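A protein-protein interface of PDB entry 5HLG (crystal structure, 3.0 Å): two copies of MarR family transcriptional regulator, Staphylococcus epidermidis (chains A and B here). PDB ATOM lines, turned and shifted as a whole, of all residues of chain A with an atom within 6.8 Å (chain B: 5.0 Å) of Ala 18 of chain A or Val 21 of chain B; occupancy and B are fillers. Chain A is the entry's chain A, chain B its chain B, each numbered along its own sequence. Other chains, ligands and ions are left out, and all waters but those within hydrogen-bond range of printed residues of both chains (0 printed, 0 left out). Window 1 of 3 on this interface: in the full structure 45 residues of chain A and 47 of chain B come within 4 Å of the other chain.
The side-chain hydroxyl (OG) of Ser 22 of chain A sits close to the side-chain hydroxyl (OG) of Ser 22 of chain B, 3.4 Å away.
OE2 of Glu 139 of chain A lies within hydrogen-bond range of ND2 of Asn 20 of chain B (3.4 Å).
The backbone NH (N) of Tyr 19 of chain A sits close to the side-chain hydroxyl (OG) of Ser 22 of chain B (3.4 Å).
The backbone carbonyl oxygen of Tyr 19 of chain A sits at hydrogen-bond distance from the side-chain hydroxyl of Ser 22 of chain A (3.2 Å).
The side-chain amide oxygen (OD1) of Asn 20 of chain B lies within hydrogen-bond range of the guanidinium group (NH1) of Arg 23 of chain B.
The side-chain hydroxyl (OG) of Ser 17 of chain A is in hydrogen-bond range of the backbone carbonyl oxygen (O) of Gln 13 of chain A, at 2.8 Å.
The backbone carbonyl oxygen (O) of Ala 18 of chain A sits at hydrogen-bond distance from the side-chain hydroxyl (OG) of Ser 22 of chain A (3.1 Å).
The guanidinium group (NH1) of Arg 23 of chain A lies within hydrogen-bond range of the side-chain hydroxyl (OH) of Tyr 19 of chain A, at 3.3 Å.
Of chain B, only Val 21, Ser 22, Phe 25 and Phe 135 come within 4 Å of Ala 18 of chain A.
Arg 23 of chain A touches none of the printed residues of chain B.
Printed residues of chain B within 4 Å of Glu 139 of chain A: Ser 17, Asn 20 and Leu 24.
Of the printed residues of chain B, Leu 142 of chain A touches Val 21, Leu 24 and Phe 25.
Of the printed residues of chain A, Ala 18 of chain B touches Val 21, Ser 22 and Phe 135.
Of chain A, only Ala 18, Phe 135, Leu 138 and Leu 142 come within 4 Å of Val 21 of chain B.
Printed residues of chain A within 4 Å of Ser 22 of chain B: Ala 18, Tyr 19 and Ser 22.
Arg 23 of chain B touches none of the printed residues of chain A.
Of the printed residues of chain A, Leu 24 of chain B touches Glu 139 (3.6 Å) and Leu 142 (3.8 Å).
The nearest residue of chain B that does not touch Ala 18 of chain A is Ala 18 of chain B (4.5 Å).
The nearest printed residue of chain A that does not touch Ser 17 of chain B is Glu 136 of chain A (4.4 Å).
Printed residues of chain A that touch a printed residue of chain B: Leu 14, Cys 15, Ser 17, Ala 18, Tyr 19, Val 21, Ser 22, Phe 135, Leu 138, Glu 139 and Leu 142.
Hydrophobic or aromatic side chains of chain A within 4 Å of the printed part of chain B: Leu 14, Ala 18, Val 21, Phe 135, Leu 138 and Leu 142.
Printed residues of chain B that touch a printed residue of chain A: Ser 17, Ala 18, Asn 20, Val 21, Ser 22, Leu 24, Phe 25 and Phe 135.
Along chain B the printed residues that touch a printed residue of chain A span positions 17 to 135.
Among the printed residues, 23 pairs touch across the chains.
Ser 17 of chain A touches Phe 135 of chain B, and with the chains exchanged Phe 135 of chain A touches Ser 17 of chain B.
Ala 18 of chain A touches Val 21 of chain B, and with the chains exchanged Val 21 of chain A touches Ala 18 of chain B.
Ala 18 of chain A touches Phe 135 of chain B, and with the chains exchanged Phe 135 of chain A touches Ala 18 of chain B.
Tyr 19 of chain A touches Ser 22 of chain B, but with the chains exchanged Ser 22 of chain A does not touch Tyr 19 of chain B (4.3 Å).
Leu 14 of chain A touches Phe 25 of chain B (O to CE2, 3.8 Å).
SG of Cys 15 of chain A touches CB of Phe 25 of chain B (3.6 Å).
Ala 18 of chain A touches Ser 22 of chain B (O to OG, 3.5 Å).
Ala 18 of chain A touches Phe 135 of chain B (CB to CE2, 3.8 Å).
Phe 135 of chain A touches Ala 18 of chain B.
CZ of Phe 135 of chain A touches CE2 of Phe 135 of chain B, 3.4 Å away.
Val 21 of chain B touches Leu 138 of chain A (CG1 to CD2, 3.8 Å).
Glu 139 of chain A touches Ser 17 of chain B.
Leu 142 of chain A touches Val 21 of chain B (CD1 to O, 3.7 Å).
Leu 142 of chain A touches Phe 25 of chain B.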
ATOM      1  N   ASN A  12     -22.182 -21.708  19.521  1.00  0.00           N
ATOM      2  CA  ASN A  12     -21.013 -22.442  19.057  1.00  0.00           C
ATOM      3  C   ASN A  12     -19.824 -22.355  20.018  1.00  0.00           C
ATOM      4  O   ASN A  12     -19.218 -23.365  20.364  1.00  0.00           O
ATOM      5  CB  ASN A  12     -20.591 -21.942  17.670  1.00  0.00           C
ATOM      6  CG  ASN A  12     -21.463 -22.488  16.563  1.00  0.00           C
ATOM      7  OD1 ASN A  12     -22.313 -23.363  16.787  1.00  0.00           O
ATOM      8  ND2 ASN A  12     -21.245 -21.984  15.346  1.00  0.00           N
ATOM      9  N   GLN A  13     -19.486 -21.150  20.445  1.00  0.00           N
ATOM     10  CA  GLN A  13     -18.368 -20.988  21.379  1.00  0.00           C
ATOM     11  C   GLN A  13     -18.711 -21.705  22.674  1.00  0.00           C
ATOM     12  O   GLN A  13     -17.837 -22.265  23.342  1.00  0.00           O
ATOM     13  CB  GLN A  13     -18.049 -19.507  21.686  1.00  0.00           C
ATOM     14  CG  GLN A  13     -17.588 -18.643  20.508  1.00  0.00           C
ATOM     15  CD  GLN A  13     -17.418 -17.155  20.858  1.00  0.00           C
ATOM     16  OE1 GLN A  13     -18.116 -16.630  21.723  1.00  0.00           O
ATOM     17  NE2 GLN A  13     -16.520 -16.461  20.144  1.00  0.00           N
ATOM     18  N   LEU A  14     -19.990 -21.695  23.020  1.00  0.00           N
ATOM     19  CA  LEU A  14     -20.447 -22.269  24.266  1.00  0.00           C
ATOM     20  C   LEU A  14     -20.469 -23.789  24.191  1.00  0.00           C
ATOM     21  O   LEU A  14     -20.097 -24.488  25.142  1.00  0.00           O
ATOM     22  CB  LEU A  14     -21.839 -21.724  24.584  1.00  0.00           C
ATOM     23  CG  LEU A  14     -22.439 -22.118  25.927  1.00  0.00           C
ATOM     24  CD1 LEU A  14     -21.640 -21.497  27.060  1.00  0.00           C
ATOM     25  CD2 LEU A  14     -23.901 -21.694  25.994  1.00  0.00           C
ATOM     26  N   CYS A  15     -20.920 -24.295  23.051  1.00  0.00           N
ATOM     27  CA  CYS A  15     -20.898 -25.726  22.776  1.00  0.00           C
ATOM     28  C   CYS A  15     -19.452 -26.207  22.794  1.00  0.00           C
ATOM     29  O   CYS A  15     -19.094 -27.134  23.517  1.00  0.00           O
ATOM     30  CB  CYS A  15     -21.546 -25.992  21.411  1.00  0.00           C
ATOM     31  SG  CYS A  15     -21.826 -27.733  21.062  1.00  0.00           S
ATOM     32  N   PHE A  16     -18.616 -25.514  22.030  1.00  0.00           N
ATOM     33  CA  PHE A  16     -17.210 -25.859  21.902  1.00  0.00           C
ATOM     34  C   PHE A  16     -16.467 -25.824  23.235  1.00  0.00           C
ATOM     35  O   PHE A  16     -15.601 -26.664  23.492  1.00  0.00           O
ATOM     36  CB  PHE A  16     -16.555 -24.918  20.883  1.00  0.00           C
ATOM     37  CG  PHE A  16     -15.121 -25.228  20.595  1.00  0.00           C
ATOM     38  CD1 PHE A  16     -14.689 -26.540  20.420  1.00  0.00           C
ATOM     39  CD2 PHE A  16     -14.203 -24.200  20.459  1.00  0.00           C
ATOM     40  CE1 PHE A  16     -13.360 -26.820  20.151  1.00  0.00           C
ATOM     41  CE2 PHE A  16     -12.877 -24.470  20.184  1.00  0.00           C
ATOM     42  CZ  PHE A  16     -12.454 -25.780  20.031  1.00  0.00           C
ATOM     43  N   SER A  17     -16.794 -24.849  24.080  1.00  0.00           N
ATOM     44  CA  SER A  17     -16.191 -24.777  25.401  1.00  0.00           C
ATOM     45  C   SER A  17     -16.583 -25.969  26.263  1.00  0.00           C
ATOM     46  O   SER A  17     -15.748 -26.569  26.936  1.00  0.00           O
ATOM     47  CB  SER A  17     -16.580 -23.488  26.123  1.00  0.00           C
ATOM     48  OG  SER A  17     -16.044 -22.362  25.440  1.00  0.00           O
ATOM     49  N   ALA A  18     -17.859 -26.310  26.247  1.00  0.00           N
ATOM     50  CA  ALA A  18     -18.338 -27.443  27.016  1.00  0.00           C
ATOM     51  C   ALA A  18     -17.629 -28.703  26.554  1.00  0.00           C
ATOM     52  O   ALA A  18     -17.225 -29.513  27.402  1.00  0.00           O
ATOM     53  CB  ALA A  18     -19.851 -27.585  26.900  1.00  0.00           C
ATOM     54  N   TYR A  19     -17.457 -28.823  25.222  1.00  0.00           N
ATOM     55  CA  TYR A  19     -16.712 -29.912  24.584  1.00  0.00           C
ATOM     56  C   TYR A  19     -15.299 -29.989  25.134  1.00  0.00           C
ATOM     57  O   TYR A  19     -14.864 -31.054  25.545  1.00  0.00           O
ATOM     58  CB  TYR A  19     -16.649 -29.678  23.071  1.00  0.00           C
ATOM     59  CG  TYR A  19     -15.897 -30.714  22.246  1.00  0.00           C
ATOM     60  CD1 TYR A  19     -16.349 -32.018  22.151  1.00  0.00           C
ATOM     61  CD2 TYR A  19     -14.764 -30.365  21.517  1.00  0.00           C
ATOM     62  CE1 TYR A  19     -15.679 -32.954  21.384  1.00  0.00           C
ATOM     63  CE2 TYR A  19     -14.086 -31.298  20.747  1.00  0.00           C
ATOM     64  CZ  TYR A  19     -14.552 -32.586  20.686  1.00  0.00           C
ATOM     65  OH  TYR A  19     -13.895 -33.515  19.930  1.00  0.00           O
ATOM     66  N   ASN A  20     -14.592 -28.860  25.124  1.00  0.00           N
ATOM     67  CA  ASN A  20     -13.229 -28.793  25.664  1.00  0.00           C
ATOM     68  C   ASN A  20     -13.142 -29.049  27.164  1.00  0.00           C
ATOM     69  O   ASN A  20     -12.262 -29.782  27.619  1.00  0.00           O
ATOM     70  CB  ASN A  20     -12.599 -27.445  25.336  1.00  0.00           C
ATOM     71  CG  ASN A  20     -12.306 -27.281  23.851  1.00  0.00           C
ATOM     72  OD1 ASN A  20     -12.134 -28.259  23.119  1.00  0.00           O
ATOM     73  ND2 ASN A  20     -12.248 -26.033  23.401  1.00  0.00           N
ATOM     74  N   VAL A  21     -14.059 -28.462  27.929  1.00  0.00           N
ATOM     75  CA  VAL A  21     -14.068 -28.630  29.378  1.00  0.00           C
ATOM     76  C   VAL A  21     -14.218 -30.096  29.793  1.00  0.00           C
ATOM     77  O   VAL A  21     -13.483 -30.590  30.641  1.00  0.00           O
ATOM     78  CB  VAL A  21     -15.167 -27.761  30.033  1.00  0.00           C
ATOM     79  CG1 VAL A  21     -15.446 -28.192  31.472  1.00  0.00           C
ATOM     80  CG2 VAL A  21     -14.754 -26.301  29.998  1.00  0.00           C
ATOM     81  N   SER A  22     -15.176 -30.792  29.208  1.00  0.00           N
ATOM     82  CA  SER A  22     -15.435 -32.183  29.622  1.00  0.00           C
ATOM     83  C   SER A  22     -14.260 -33.087  29.253  1.00  0.00           C
ATOM     84  O   SER A  22     -13.913 -33.990  30.020  1.00  0.00           O
ATOM     85  CB  SER A  22     -16.758 -32.729  29.048  1.00  0.00           C
ATOM     86  OG  SER A  22     -16.772 -32.560  27.641  1.00  0.00           O
ATOM     87  N   ARG A  23     -13.613 -32.824  28.113  1.00  0.00           N
ATOM     88  CA  ARG A  23     -12.448 -33.625  27.716  1.00  0.00           C
ATOM     89  C   ARG A  23     -11.316 -33.427  28.716  1.00  0.00           C
ATOM     90  O   ARG A  23     -10.672 -34.405  29.143  1.00  0.00           O
ATOM     91  CB  ARG A  23     -11.973 -33.267  26.311  1.00  0.00           C
ATOM     92  CG  ARG A  23     -13.033 -33.508  25.262  1.00  0.00           C
ATOM     93  CD  ARG A  23     -12.485 -33.507  23.862  1.00  0.00           C
ATOM     94  NE  ARG A  23     -11.631 -32.298  23.671  1.00  0.00           N
ATOM     95  CZ  ARG A  23     -11.017 -31.994  22.546  1.00  0.00           C
ATOM     96  NH1 ARG A  23     -11.110 -32.786  21.499  1.00  0.00           N
ATOM     97  NH2 ARG A  23     -10.314 -30.896  22.461  1.00  0.00           N
ATOM     98  N   VAL A 134     -24.415 -22.246  37.134  1.00  0.00           N
ATOM     99  CA  VAL A 134     -24.478 -21.897  35.703  1.00  0.00           C
ATOM    100  C   VAL A 134     -24.547 -23.124  34.789  1.00  0.00           C
ATOM    101  O   VAL A 134     -25.205 -23.098  33.743  1.00  0.00           O
ATOM    102  CB  VAL A 134     -23.261 -21.045  35.284  1.00  0.00           C
ATOM    103  CG1 VAL A 134     -23.174 -20.918  33.770  1.00  0.00           C
ATOM    104  CG2 VAL A 134     -23.331 -19.668  35.919  1.00  0.00           C
ATOM    105  N   PHE A 135     -23.841 -24.182  35.175  1.00  0.00           N
ATOM    106  CA  PHE A 135     -23.893 -25.454  34.462  1.00  0.00           C
ATOM    107  C   PHE A 135     -25.283 -26.078  34.570  1.00  0.00           C
ATOM    108  O   PHE A 135     -25.903 -26.382  33.546  1.00  0.00           O
ATOM    109  CB  PHE A 135     -22.825 -26.422  34.985  1.00  0.00           C
ATOM    110  CG  PHE A 135     -21.476 -26.260  34.327  1.00  0.00           C
ATOM    111  CD1 PHE A 135     -20.681 -25.161  34.603  1.00  0.00           C
ATOM    112  CD2 PHE A 135     -20.997 -27.218  33.443  1.00  0.00           C
ATOM    113  CE1 PHE A 135     -19.438 -25.015  34.004  1.00  0.00           C
ATOM    114  CE2 PHE A 135     -19.755 -27.076  32.841  1.00  0.00           C
ATOM    115  CZ  PHE A 135     -18.975 -25.973  33.123  1.00  0.00           C
ATOM    116  N   GLU A 136     -25.770 -26.250  35.804  1.00  0.00           N
ATOM    117  CA  GLU A 136     -27.107 -26.819  36.042  1.00  0.00           C
ATOM    118  C   GLU A 136     -28.219 -26.071  35.294  1.00  0.00           C
ATOM    119  O   GLU A 136     -29.200 -26.677  34.854  1.00  0.00           O
ATOM    120  CB  GLU A 136     -27.410 -26.890  37.545  1.00  0.00           C
ATOM    121  CG  GLU A 136     -26.827 -28.128  38.216  1.00  0.00           C
ATOM    122  CD  GLU A 136     -26.706 -27.991  39.720  1.00  0.00           C
ATOM    123  OE1 GLU A 136     -27.076 -28.953  40.427  1.00  0.00           O
ATOM    124  OE2 GLU A 136     -26.240 -26.932  40.196  1.00  0.00           O
ATOM    125  N   LEU A 138     -27.865 -24.416  32.304  1.00  0.00           N
ATOM    126  CA  LEU A 138     -27.699 -24.815  30.913  1.00  0.00           C
ATOM    127  C   LEU A 138     -28.056 -26.275  30.700  1.00  0.00           C
ATOM    128  O   LEU A 138     -28.580 -26.632  29.655  1.00  0.00           O
ATOM    129  CB  LEU A 138     -26.254 -24.585  30.487  1.00  0.00           C
ATOM    130  CG  LEU A 138     -25.887 -24.942  29.053  1.00  0.00           C
ATOM    131  CD1 LEU A 138     -26.690 -24.132  28.053  1.00  0.00           C
ATOM    132  CD2 LEU A 138     -24.400 -24.718  28.858  1.00  0.00           C
ATOM    133  N   GLU A 139     -27.740 -27.111  31.685  1.00  0.00           N
ATOM    134  CA  GLU A 139     -28.109 -28.521  31.678  1.00  0.00           C
ATOM    135  C   GLU A 139     -29.621 -28.657  31.509  1.00  0.00           C
ATOM    136  O   GLU A 139     -30.099 -29.374  30.633  1.00  0.00           O
ATOM    137  CB  GLU A 139     -27.651 -29.181  32.982  1.00  0.00           C
ATOM    138  CG  GLU A 139     -27.652 -30.698  32.991  1.00  0.00           C
ATOM    139  CD  GLU A 139     -27.128 -31.266  34.306  1.00  0.00           C
ATOM    140  OE1 GLU A 139     -26.276 -30.621  34.964  1.00  0.00           O
ATOM    141  OE2 GLU A 139     -27.583 -32.360  34.697  1.00  0.00           O
ATOM    142  N   GLN A 140     -30.369 -27.942  32.338  1.00  0.00           N
ATOM    143  CA  GLN A 140     -31.835 -27.968  32.267  1.00  0.00           C
ATOM    144  C   GLN A 140     -32.389 -27.293  31.002  1.00  0.00           C
ATOM    145  O   GLN A 140     -33.401 -27.743  30.463  1.00  0.00           O
ATOM    146  CB  GLN A 140     -32.483 -27.425  33.561  1.00  0.00           C
ATOM    147  CG  GLN A 140     -33.818 -28.050  33.905  1.00  0.00           C
ATOM    148  CD  GLN A 140     -34.293 -27.724  35.309  1.00  0.00           C
ATOM    149  OE1 GLN A 140     -33.541 -27.204  36.136  1.00  0.00           O
ATOM    150  NE2 GLN A 140     -35.550 -28.047  35.588  1.00  0.00           N
ATOM    151  N   LEU A 142     -30.889 -27.250  28.005  1.00  0.00           N
ATOM    152  CA  LEU A 142     -30.639 -28.200  26.931  1.00  0.00           C
ATOM    153  C   LEU A 142     -31.609 -29.380  26.986  1.00  0.00           C
ATOM    154  O   LEU A 142     -32.148 -29.772  25.952  1.00  0.00           O
ATOM    155  CB  LEU A 142     -29.181 -28.681  26.970  1.00  0.00           C
ATOM    156  CG  LEU A 142     -28.120 -27.657  26.557  1.00  0.00           C
ATOM    157  CD1 LEU A 142     -26.735 -28.145  26.942  1.00  0.00           C
ATOM    158  CD2 LEU A 142     -28.175 -27.383  25.063  1.00  0.00           C
ATOM    159  N   SER B  17     -21.412 -32.267  35.936  1.00  0.00           N
ATOM    160  CA  SER B  17     -22.245 -31.325  35.192  1.00  0.00           C
ATOM    161  C   SER B  17     -21.688 -31.063  33.804  1.00  0.00           C
ATOM    162  O   SER B  17     -22.436 -31.037  32.830  1.00  0.00           O
ATOM    163  CB  SER B  17     -22.386 -29.996  35.938  1.00  0.00           C
ATOM    164  OG  SER B  17     -23.084 -30.172  37.156  1.00  0.00           O
ATOM    165  N   ALA B  18     -20.377 -30.836  33.724  1.00  0.00           N
ATOM    166  CA  ALA B  18     -19.716 -30.607  32.436  1.00  0.00           C
ATOM    167  C   ALA B  18     -19.845 -31.820  31.522  1.00  0.00           C
ATOM    168  O   ALA B  18     -19.972 -31.679  30.304  1.00  0.00           O
ATOM    169  CB  ALA B  18     -18.251 -30.271  32.645  1.00  0.00           C
ATOM    170  N   TYR B  19     -19.793 -33.004  32.127  1.00  0.00           N
ATOM    171  CA  TYR B  19     -20.042 -34.267  31.438  1.00  0.00           C
ATOM    172  C   TYR B  19     -21.427 -34.169  30.821  1.00  0.00           C
ATOM    173  O   TYR B  19     -21.546 -34.158  29.594  1.00  0.00           O
ATOM    174  CB  TYR B  19     -19.921 -35.433  32.432  1.00  0.00           C
ATOM    175  CG  TYR B  19     -20.166 -36.832  31.891  1.00  0.00           C
ATOM    176  CD1 TYR B  19     -19.307 -37.407  30.957  1.00  0.00           C
ATOM    177  CD2 TYR B  19     -21.225 -37.610  32.368  1.00  0.00           C
ATOM    178  CE1 TYR B  19     -19.519 -38.701  30.487  1.00  0.00           C
ATOM    179  CE2 TYR B  19     -21.442 -38.909  31.907  1.00  0.00           C
ATOM    180  CZ  TYR B  19     -20.592 -39.449  30.966  1.00  0.00           C
ATOM    181  OH  TYR B  19     -20.823 -40.729  30.526  1.00  0.00           O
ATOM    182  N   ASN B  20     -22.450 -33.994  31.663  1.00  0.00           N
ATOM    183  CA  ASN B  20     -23.842 -33.945  31.194  1.00  0.00           C
ATOM    184  C   ASN B  20     -24.101 -32.852  30.147  1.00  0.00           C
ATOM    185  O   ASN B  20     -24.776 -33.084  29.136  1.00  0.00           O
ATOM    186  CB  ASN B  20     -24.804 -33.753  32.371  1.00  0.00           C
ATOM    187  CG  ASN B  20     -24.968 -34.999  33.222  1.00  0.00           C
ATOM    188  OD1 ASN B  20     -24.914 -36.119  32.725  1.00  0.00           O
ATOM    189  ND2 ASN B  20     -25.231 -34.803  34.509  1.00  0.00           N
ATOM    190  N   VAL B  21     -23.563 -31.666  30.388  1.00  0.00           N
ATOM    191  CA  VAL B  21     -23.759 -30.546  29.477  1.00  0.00           C
ATOM    192  C   VAL B  21     -23.226 -30.837  28.083  1.00  0.00           C
ATOM    193  O   VAL B  21     -23.911 -30.557  27.108  1.00  0.00           O
ATOM    194  CB  VAL B  21     -23.117 -29.256  30.022  1.00  0.00           C
ATOM    195  CG1 VAL B  21     -22.971 -28.196  28.931  1.00  0.00           C
ATOM    196  CG2 VAL B  21     -23.954 -28.720  31.169  1.00  0.00           C
ATOM    197  N   SER B  22     -22.012 -31.381  27.981  1.00  0.00           N
ATOM    198  CA  SER B  22     -21.430 -31.628  26.669  1.00  0.00           C
ATOM    199  C   SER B  22     -22.177 -32.715  25.907  1.00  0.00           C
ATOM    200  O   SER B  22     -22.355 -32.599  24.691  1.00  0.00           O
ATOM    201  CB  SER B  22     -19.962 -31.971  26.792  1.00  0.00           C
ATOM    202  OG  SER B  22     -19.295 -31.701  25.562  1.00  0.00           O
ATOM    203  N   ARG B  23     -22.630 -33.744  26.615  1.00  0.00           N
ATOM    204  CA  ARG B  23     -23.414 -34.808  25.999  1.00  0.00           C
ATOM    205  C   ARG B  23     -24.712 -34.250  25.422  1.00  0.00           C
ATOM    206  O   ARG B  23     -25.108 -34.600  24.309  1.00  0.00           O
ATOM    207  CB  ARG B  23     -23.719 -35.909  27.017  1.00  0.00           C
ATOM    208  CG  ARG B  23     -22.499 -36.413  27.771  1.00  0.00           C
ATOM    209  CD  ARG B  23     -22.547 -37.921  27.952  1.00  0.00           C
ATOM    210  NE  ARG B  23     -23.818 -38.364  28.518  1.00  0.00           N
ATOM    211  CZ  ARG B  23     -24.220 -38.091  29.756  1.00  0.00           C
ATOM    212  NH1 ARG B  23     -23.449 -37.374  30.562  1.00  0.00           N
ATOM    213  NH2 ARG B  23     -25.392 -38.535  30.186  1.00  0.00           N
ATOM    214  N   LEU B  24     -25.368 -33.381  26.185  1.00  0.00           N
ATOM    215  CA  LEU B  24     -26.608 -32.750  25.746  1.00  0.00           C
ATOM    216  C   LEU B  24     -26.389 -31.842  24.537  1.00  0.00           C
ATOM    217  O   LEU B  24     -27.108 -31.922  23.539  1.00  0.00           O
ATOM    218  CB  LEU B  24     -27.256 -31.985  26.900  1.00  0.00           C
ATOM    219  CG  LEU B  24     -27.788 -32.888  28.027  1.00  0.00           C
ATOM    220  CD1 LEU B  24     -28.083 -32.100  29.294  1.00  0.00           C
ATOM    221  CD2 LEU B  24     -29.028 -33.644  27.582  1.00  0.00           C
ATOM    222  N   PHE B  25     -25.392 -30.982  24.610  1.00  0.00           N
ATOM    223  CA  PHE B  25     -25.012 -30.192  23.432  1.00  0.00           C
ATOM    224  C   PHE B  25     -24.784 -31.028  22.175  1.00  0.00           C
ATOM    225  O   PHE B  25     -25.167 -30.622  21.071  1.00  0.00           O
ATOM    226  CB  PHE B  25     -23.735 -29.392  23.682  1.00  0.00           C
ATOM    227  CG  PHE B  25     -23.976 -27.953  24.044  1.00  0.00           C
ATOM    228  CD1 PHE B  25     -24.806 -27.148  23.263  1.00  0.00           C
ATOM    229  CD2 PHE B  25     -23.359 -27.396  25.144  1.00  0.00           C
ATOM    230  CE1 PHE B  25     -25.032 -25.822  23.586  1.00  0.00           C
ATOM    231  CE2 PHE B  25     -23.575 -26.070  25.468  1.00  0.00           C
ATOM    232  CZ  PHE B  25     -24.409 -25.282  24.689  1.00  0.00           C
ATOM    233  N   PHE B 135     -17.094 -20.592  31.485  1.00  0.00           N
ATOM    234  CA  PHE B 135     -16.542 -21.780  30.847  1.00  0.00           C
ATOM    235  C   PHE B 135     -15.068 -21.545  30.538  1.00  0.00           C
ATOM    236  O   PHE B 135     -14.199 -22.241  31.081  1.00  0.00           O
ATOM    237  CB  PHE B 135     -17.344 -22.151  29.593  1.00  0.00           C
ATOM    238  CG  PHE B 135     -18.528 -23.020  29.881  1.00  0.00           C
ATOM    239  CD1 PHE B 135     -19.652 -22.503  30.508  1.00  0.00           C
ATOM    240  CD2 PHE B 135     -18.510 -24.365  29.551  1.00  0.00           C
ATOM    241  CE1 PHE B 135     -20.744 -23.310  30.784  1.00  0.00           C
ATOM    242  CE2 PHE B 135     -19.596 -25.171  29.827  1.00  0.00           C
ATOM    243  CZ  PHE B 135     -20.715 -24.649  30.441  1.00  0.00           C
